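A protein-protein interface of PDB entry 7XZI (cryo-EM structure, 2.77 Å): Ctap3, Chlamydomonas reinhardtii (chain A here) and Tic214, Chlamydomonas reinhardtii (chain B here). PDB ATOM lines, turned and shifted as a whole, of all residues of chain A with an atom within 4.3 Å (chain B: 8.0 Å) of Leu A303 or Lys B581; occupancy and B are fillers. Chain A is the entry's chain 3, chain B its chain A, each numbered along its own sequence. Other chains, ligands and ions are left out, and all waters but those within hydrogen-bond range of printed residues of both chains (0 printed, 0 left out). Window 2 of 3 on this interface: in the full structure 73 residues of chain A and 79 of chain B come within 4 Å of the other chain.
CE1 of Tyr A299 touches CG of Leu B679, 3.6 Å away.
Lys B581 touches Val A302.
CD2 of Leu A303 touches CD1 of Leu B578, at 3.7 Å.
Lys B581 touches Leu A303.
CD of Arg B577 touches OE1 of Gln A310, 3.4 Å away.
Glu A300 touches none of the printed residues of chain B.
Leu A303 touches two residues of chain B.
No residue of chain B comes within 4 Å of Gly A304.
Printed residues of chain B within 4 Å of Gln A310: Arg B577.
Lys B581 touches just these residues of chain A: Val A302 and Leu A303.
Printed residues of chain A within 4 Å of Leu B679: Tyr A299.
The nearest residue of chain B that does not touch Leu A303 is Arg B577 (4.1 Å).
The nearest printed residue of chain A that does not touch Lys B581 is Gly A304 (4.9 Å).
Hydrophobic or aromatic side chains of chain B within 4 Å of the printed part of chain A: Leu B578 and Leu B679.
Hydrophobic or aromatic side chains of chain A within 4 Å of the printed part of chain B: Tyr A299 and Leu A303.
Among the printed residues, 5 pairs touch across the chains.
Among the printed residues, no Asp or Glu carboxylate lies within 4 Å of a Lys or Arg side-chain nitrogen of the other chain.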
ATOM      1  N   TYR A 299      10.857 -15.969 -25.461  1.00  0.00           N
ATOM      2  CA  TYR A 299      10.075 -16.232 -26.665  1.00  0.00           C
ATOM      3  C   TYR A 299       9.148 -17.423 -26.468  1.00  0.00           C
ATOM      4  O   TYR A 299       7.968 -17.375 -26.837  1.00  0.00           O
ATOM      5  CB  TYR A 299      11.004 -16.473 -27.855  1.00  0.00           C
ATOM      6  CG  TYR A 299      11.734 -15.244 -28.344  1.00  0.00           C
ATOM      7  CD1 TYR A 299      11.375 -13.977 -27.905  1.00  0.00           C
ATOM      8  CD2 TYR A 299      12.776 -15.352 -29.254  1.00  0.00           C
ATOM      9  CE1 TYR A 299      12.041 -12.852 -28.353  1.00  0.00           C
ATOM     10  CE2 TYR A 299      13.446 -14.233 -29.710  1.00  0.00           C
ATOM     11  CZ  TYR A 299      13.075 -12.986 -29.256  1.00  0.00           C
ATOM     12  OH  TYR A 299      13.741 -11.871 -29.708  1.00  0.00           O
ATOM     13  N   GLU A 300       9.667 -18.509 -25.889  1.00  0.00           N
ATOM     14  CA  GLU A 300       8.842 -19.694 -25.677  1.00  0.00           C
ATOM     15  C   GLU A 300       7.726 -19.433 -24.675  1.00  0.00           C
ATOM     16  O   GLU A 300       6.660 -20.051 -24.762  1.00  0.00           O
ATOM     17  CB  GLU A 300       9.707 -20.867 -25.219  1.00  0.00           C
ATOM     18  CG  GLU A 300      10.663 -21.384 -26.281  1.00  0.00           C
ATOM     19  CD  GLU A 300      11.428 -22.609 -25.825  1.00  0.00           C
ATOM     20  OE1 GLU A 300      11.149 -23.103 -24.712  1.00  0.00           O
ATOM     21  OE2 GLU A 300      12.307 -23.079 -26.578  1.00  0.00           O
ATOM     22  N   ALA A 301       7.952 -18.538 -23.713  1.00  0.00           N
ATOM     23  CA  ALA A 301       6.900 -18.196 -22.764  1.00  0.00           C
ATOM     24  C   ALA A 301       5.826 -17.334 -23.417  1.00  0.00           C
ATOM     25  O   ALA A 301       4.627 -17.559 -23.218  1.00  0.00           O
ATOM     26  CB  ALA A 301       7.498 -17.486 -21.549  1.00  0.00           C
ATOM     27  N   VAL A 302       6.238 -16.334 -24.199  1.00  0.00           N
ATOM     28  CA  VAL A 302       5.271 -15.387 -24.746  1.00  0.00           C
ATOM     29  C   VAL A 302       4.473 -16.005 -25.890  1.00  0.00           C
ATOM     30  O   VAL A 302       3.262 -15.783 -26.000  1.00  0.00           O
ATOM     31  CB  VAL A 302       5.973 -14.081 -25.170  1.00  0.00           C
ATOM     32  CG1 VAL A 302       6.941 -14.315 -26.322  1.00  0.00           C
ATOM     33  CG2 VAL A 302       4.945 -13.020 -25.536  1.00  0.00           C
ATOM     34  N   LEU A 303       5.119 -16.790 -26.759  1.00  0.00           N
ATOM     35  CA  LEU A 303       4.472 -17.281 -27.968  1.00  0.00           C
ATOM     36  C   LEU A 303       4.335 -18.795 -28.041  1.00  0.00           C
ATOM     37  O   LEU A 303       3.525 -19.282 -28.834  1.00  0.00           O
ATOM     38  CB  LEU A 303       5.234 -16.800 -29.213  1.00  0.00           C
ATOM     39  CG  LEU A 303       5.109 -15.311 -29.532  1.00  0.00           C
ATOM     40  CD1 LEU A 303       5.981 -14.929 -30.717  1.00  0.00           C
ATOM     41  CD2 LEU A 303       3.656 -14.964 -29.798  1.00  0.00           C
ATOM     42  N   GLY A 304       5.092 -19.540 -27.253  1.00  0.00           N
ATOM     43  CA  GLY A 304       5.082 -20.986 -27.322  1.00  0.00           C
ATOM     44  C   GLY A 304       6.336 -21.521 -27.990  1.00  0.00           C
ATOM     45  O   GLY A 304       7.276 -20.788 -28.306  1.00  0.00           O
ATOM     46  N   TRP A 307       7.618 -20.364 -32.035  1.00  0.00           N
ATOM     47  CA  TRP A 307       7.617 -18.923 -32.261  1.00  0.00           C
ATOM     48  C   TRP A 307       8.180 -18.566 -33.632  1.00  0.00           C
ATOM     49  O   TRP A 307       7.700 -17.621 -34.272  1.00  0.00           O
ATOM     50  CB  TRP A 307       8.398 -18.215 -31.153  1.00  0.00           C
ATOM     51  CG  TRP A 307       9.724 -18.838 -30.836  1.00  0.00           C
ATOM     52  CD1 TRP A 307       9.953 -19.928 -30.046  1.00  0.00           C
ATOM     53  CD2 TRP A 307      11.011 -18.394 -31.284  1.00  0.00           C
ATOM     54  NE1 TRP A 307      11.298 -20.196 -29.985  1.00  0.00           N
ATOM     55  CE2 TRP A 307      11.970 -19.267 -30.735  1.00  0.00           C
ATOM     56  CE3 TRP A 307      11.444 -17.345 -32.101  1.00  0.00           C
ATOM     57  CZ2 TRP A 307      13.334 -19.125 -30.976  1.00  0.00           C
ATOM     58  CZ3 TRP A 307      12.797 -17.206 -32.337  1.00  0.00           C
ATOM     59  CH2 TRP A 307      13.727 -18.090 -31.779  1.00  0.00           C
ATOM     60  N   GLN A 310       5.510 -18.845 -36.333  1.00  0.00           N
ATOM     61  CA  GLN A 310       4.560 -17.739 -36.264  1.00  0.00           C
ATOM     62  C   GLN A 310       5.162 -16.451 -36.819  1.00  0.00           C
ATOM     63  O   GLN A 310       4.486 -15.703 -37.535  1.00  0.00           O
ATOM     64  CB  GLN A 310       4.095 -17.539 -34.823  1.00  0.00           C
ATOM     65  CG  GLN A 310       3.366 -18.739 -34.247  1.00  0.00           C
ATOM     66  CD  GLN A 310       2.938 -18.528 -32.809  1.00  0.00           C
ATOM     67  OE1 GLN A 310       3.122 -17.450 -32.244  1.00  0.00           O
ATOM     68  NE2 GLN A 310       2.365 -19.563 -32.208  1.00  0.00           N
ATOM     69  N   ASN B 573       1.583  -6.969 -37.340  1.00  0.00           N
ATOM     70  CA  ASN B 573       1.148  -8.353 -37.191  1.00  0.00           C
ATOM     71  C   ASN B 573       1.754  -8.992 -35.948  1.00  0.00           C
ATOM     72  O   ASN B 573       1.066  -9.709 -35.211  1.00  0.00           O
ATOM     73  CB  ASN B 573       1.506  -9.157 -38.441  1.00  0.00           C
ATOM     74  CG  ASN B 573       0.783  -8.663 -39.681  1.00  0.00           C
ATOM     75  OD1 ASN B 573      -0.288  -8.064 -39.594  1.00  0.00           O
ATOM     76  ND2 ASN B 573       1.368  -8.917 -40.845  1.00  0.00           N
ATOM     77  N   VAL B 574       3.042  -8.740 -35.693  1.00  0.00           N
ATOM     78  CA  VAL B 574       3.689  -9.311 -34.514  1.00  0.00           C
ATOM     79  C   VAL B 574       3.055  -8.771 -33.237  1.00  0.00           C
ATOM     80  O   VAL B 574       2.794  -9.524 -32.291  1.00  0.00           O
ATOM     81  CB  VAL B 574       5.206  -9.047 -34.553  1.00  0.00           C
ATOM     82  CG1 VAL B 574       5.845  -9.436 -33.231  1.00  0.00           C
ATOM     83  CG2 VAL B 574       5.847  -9.820 -35.692  1.00  0.00           C
ATOM     84  N   ASN B 575       2.800  -7.461 -33.187  1.00  0.00           N
ATOM     85  CA  ASN B 575       2.173  -6.879 -32.002  1.00  0.00           C
ATOM     86  C   ASN B 575       0.766  -7.430 -31.789  1.00  0.00           C
ATOM     87  O   ASN B 575       0.376  -7.737 -30.655  1.00  0.00           O
ATOM     88  CB  ASN B 575       2.143  -5.355 -32.114  1.00  0.00           C
ATOM     89  CG  ASN B 575       3.480  -4.722 -31.785  1.00  0.00           C
ATOM     90  OD1 ASN B 575       4.506  -5.397 -31.740  1.00  0.00           O
ATOM     91  ND2 ASN B 575       3.472  -3.414 -31.551  1.00  0.00           N
ATOM     92  N   THR B 576      -0.013  -7.554 -32.868  1.00  0.00           N
ATOM     93  CA  THR B 576      -1.358  -8.108 -32.755  1.00  0.00           C
ATOM     94  C   THR B 576      -1.319  -9.542 -32.247  1.00  0.00           C
ATOM     95  O   THR B 576      -2.113  -9.923 -31.380  1.00  0.00           O
ATOM     96  CB  THR B 576      -2.070  -8.048 -34.107  1.00  0.00           C
ATOM     97  OG1 THR B 576      -2.089  -6.696 -34.581  1.00  0.00           O
ATOM     98  CG2 THR B 576      -3.499  -8.557 -33.985  1.00  0.00           C
ATOM     99  N   ARG B 577      -0.398 -10.351 -32.777  1.00  0.00           N
ATOM    100  CA  ARG B 577      -0.278 -11.732 -32.323  1.00  0.00           C
ATOM    101  C   ARG B 577       0.113 -11.797 -30.854  1.00  0.00           C
ATOM    102  O   ARG B 577      -0.441 -12.600 -30.095  1.00  0.00           O
ATOM    103  CB  ARG B 577       0.740 -12.481 -33.182  1.00  0.00           C
ATOM    104  CG  ARG B 577       0.952 -13.926 -32.762  1.00  0.00           C
ATOM    105  CD  ARG B 577       1.969 -14.620 -33.649  1.00  0.00           C
ATOM    106  NE  ARG B 577       1.586 -14.573 -35.053  1.00  0.00           N
ATOM    107  CZ  ARG B 577       0.787 -15.455 -35.644  1.00  0.00           C
ATOM    108  NH1 ARG B 577       0.268 -16.472 -34.976  1.00  0.00           N
ATOM    109  NH2 ARG B 577       0.507 -15.313 -36.935  1.00  0.00           N
ATOM    110  N   LEU B 578       1.062 -10.957 -30.434  1.00  0.00           N
ATOM    111  CA  LEU B 578       1.476 -10.947 -29.033  1.00  0.00           C
ATOM    112  C   LEU B 578       0.314 -10.582 -28.120  1.00  0.00           C
ATOM    113  O   LEU B 578       0.072 -11.248 -27.106  1.00  0.00           O
ATOM    114  CB  LEU B 578       2.637  -9.972 -28.833  1.00  0.00           C
ATOM    115  CG  LEU B 578       4.016 -10.576 -28.572  1.00  0.00           C
ATOM    116  CD1 LEU B 578       4.493 -11.357 -29.783  1.00  0.00           C
ATOM    117  CD2 LEU B 578       5.015  -9.491 -28.199  1.00  0.00           C
ATOM    118  N   ASN B 579      -0.420  -9.521 -28.466  1.00  0.00           N
ATOM    119  CA  ASN B 579      -1.535  -9.092 -27.628  1.00  0.00           C
ATOM    120  C   ASN B 579      -2.631 -10.150 -27.579  1.00  0.00           C
ATOM    121  O   ASN B 579      -3.188 -10.427 -26.508  1.00  0.00           O
ATOM    122  CB  ASN B 579      -2.095  -7.761 -28.132  1.00  0.00           C
ATOM    123  CG  ASN B 579      -1.191  -6.588 -27.808  1.00  0.00           C
ATOM    124  OD1 ASN B 579      -1.237  -6.040 -26.705  1.00  0.00           O
ATOM    125  ND2 ASN B 579      -0.370  -6.187 -28.770  1.00  0.00           N
ATOM    126  N   LEU B 580      -2.956 -10.755 -28.725  1.00  0.00           N
ATOM    127  CA  LEU B 580      -3.993 -11.782 -28.750  1.00  0.00           C
ATOM    128  C   LEU B 580      -3.579 -12.998 -27.931  1.00  0.00           C
ATOM    129  O   LEU B 580      -4.392 -13.575 -27.199  1.00  0.00           O
ATOM    130  CB  LEU B 580      -4.307 -12.176 -30.195  1.00  0.00           C
ATOM    131  CG  LEU B 580      -5.556 -13.032 -30.427  1.00  0.00           C
ATOM    132  CD1 LEU B 580      -6.214 -12.660 -31.745  1.00  0.00           C
ATOM    133  CD2 LEU B 580      -5.228 -14.518 -30.403  1.00  0.00           C
ATOM    134  N   LYS B 581      -2.313 -13.409 -28.047  1.00  0.00           N
ATOM    135  CA  LYS B 581      -1.824 -14.536 -27.262  1.00  0.00           C
ATOM    136  C   LYS B 581      -1.874 -14.228 -25.771  1.00  0.00           C
ATOM    137  O   LYS B 581      -2.281 -15.077 -24.971  1.00  0.00           O
ATOM    138  CB  LYS B 581      -0.399 -14.890 -27.690  1.00  0.00           C
ATOM    139  CG  LYS B 581       0.222 -16.044 -26.921  1.00  0.00           C
ATOM    140  CD  LYS B 581      -0.347 -17.382 -27.360  1.00  0.00           C
ATOM    141  CE  LYS B 581       0.371 -18.535 -26.675  1.00  0.00           C
ATOM    142  NZ  LYS B 581      -0.102 -19.857 -27.168  1.00  0.00           N
ATOM    143  N   LEU B 582      -1.470 -13.016 -25.381  1.00  0.00           N
ATOM    144  CA  LEU B 582      -1.499 -12.645 -23.970  1.00  0.00           C
ATOM    145  C   LEU B 582      -2.922 -12.599 -23.428  1.00  0.00           C
ATOM    146  O   LEU B 582      -3.161 -13.016 -22.289  1.00  0.00           O
ATOM    147  CB  LEU B 582      -0.808 -11.294 -23.766  1.00  0.00           C
ATOM    148  CG  LEU B 582      -0.707 -10.769 -22.331  1.00  0.00           C
ATOM    149  CD1 LEU B 582       0.672 -10.185 -22.079  1.00  0.00           C
ATOM    150  CD2 LEU B 582      -1.784  -9.731 -22.047  1.00  0.00           C
ATOM    151  N   LEU B 583      -3.871 -12.098 -24.219  1.00  0.00           N
ATOM    152  CA  LEU B 583      -5.245 -11.964 -23.752  1.00  0.00           C
ATOM    153  C   LEU B 583      -5.993 -13.292 -23.716  1.00  0.00           C
ATOM    154  O   LEU B 583      -7.046 -13.376 -23.075  1.00  0.00           O
ATOM    155  CB  LEU B 583      -5.999 -10.962 -24.630  1.00  0.00           C
ATOM    156  CG  LEU B 583      -7.274 -10.354 -24.044  1.00  0.00           C
ATOM    157  CD1 LEU B 583      -7.004  -9.822 -22.648  1.00  0.00           C
ATOM    158  CD2 LEU B 583      -7.806  -9.251 -24.941  1.00  0.00           C
ATOM    159  N   ASN B 584      -5.478 -14.326 -24.383  1.00  0.00           N
ATOM    160  CA  ASN B 584      -6.127 -15.637 -24.414  1.00  0.00           C
ATOM    161  C   ASN B 584      -5.773 -16.453 -23.166  1.00  0.00           C
ATOM    162  O   ASN B 584      -5.241 -17.561 -23.234  1.00  0.00           O
ATOM    163  CB  ASN B 584      -5.745 -16.382 -25.686  1.00  0.00           C
ATOM    164  CG  ASN B 584      -6.921 -16.575 -26.622  1.00  0.00           C
ATOM    165  OD1 ASN B 584      -8.073 -16.606 -26.191  1.00  0.00           O
ATOM    166  ND2 ASN B 584      -6.636 -16.710 -27.913  1.00  0.00           N
ATOM    167  N   SER B 585      -6.083 -15.868 -22.007  1.00  0.00           N
ATOM    168  CA  SER B 585      -5.860 -16.501 -20.703  1.00  0.00           C
ATOM    169  C   SER B 585      -4.391 -16.854 -20.482  1.00  0.00           C
ATOM    170  O   SER B 585      -4.063 -17.721 -19.669  1.00  0.00           O
ATOM    171  CB  SER B 585      -6.743 -17.740 -20.527  1.00  0.00           C
ATOM    172  OG  SER B 585      -8.117 -17.398 -20.550  1.00  0.00           O
ATOM    173  N   LYS B 586      -3.489 -16.187 -21.204  1.00  0.00           N
ATOM    174  CA  LYS B 586      -2.065 -16.376 -20.964  1.00  0.00           C
ATOM    175  C   LYS B 586      -1.582 -15.614 -19.740  1.00  0.00           C
ATOM    176  O   LYS B 586      -0.508 -15.924 -19.215  1.00  0.00           O
ATOM    177  CB  LYS B 586      -1.253 -15.951 -22.186  1.00  0.00           C
ATOM    178  N   GLU B 587      -2.349 -14.624 -19.280  1.00  0.00           N
ATOM    179  CA  GLU B 587      -2.028 -13.924 -18.045  1.00  0.00           C
ATOM    180  C   GLU B 587      -2.244 -14.791 -16.813  1.00  0.00           C
ATOM    181  O   GLU B 587      -1.762 -14.435 -15.733  1.00  0.00           O
ATOM    182  CB  GLU B 587      -2.865 -12.647 -17.934  1.00  0.00           C
ATOM    183  N   LEU B 679      10.169  -7.844 -29.032  1.00  0.00           N
ATOM    184  CA  LEU B 679      10.630  -8.471 -30.266  1.00  0.00           C
ATOM    185  C   LEU B 679      10.887  -7.441 -31.361  1.00  0.00           C
ATOM    186  O   LEU B 679      11.913  -7.498 -32.047  1.00  0.00           O
ATOM    187  CB  LEU B 679       9.616  -9.513 -30.741  1.00  0.00           C
ATOM    188  CG  LEU B 679       9.526 -10.836 -29.972  1.00  0.00           C
ATOM    189  CD1 LEU B 679       8.707 -10.695 -28.694  1.00  0.00           C
ATOM    190  CD2 LEU B 679       8.963 -11.937 -30.859  1.00  0.00           C
ATOM    191  N   LEU B1181     -10.724 -13.817 -30.064  1.00  0.00           N
ATOM    192  CA  LEU B1181     -10.501 -13.962 -28.629  1.00  0.00           C
ATOM    193  C   LEU B1181     -11.259 -15.158 -28.062  1.00  0.00           C
ATOM    194  O   LEU B1181     -10.715 -15.922 -27.256  1.00  0.00           O
ATOM    195  CB  LEU B1181     -10.908 -12.685 -27.899  1.00  0.00           C
ATOM    196  CG  LEU B1181      -9.942 -11.508 -27.995  1.00  0.00           C
ATOM    197  CD1 LEU B1181     -10.464 -10.351 -27.173  1.00  0.00           C
ATOM    198  CD2 LEU B1181      -8.559 -11.922 -27.525  1.00  0.00           C
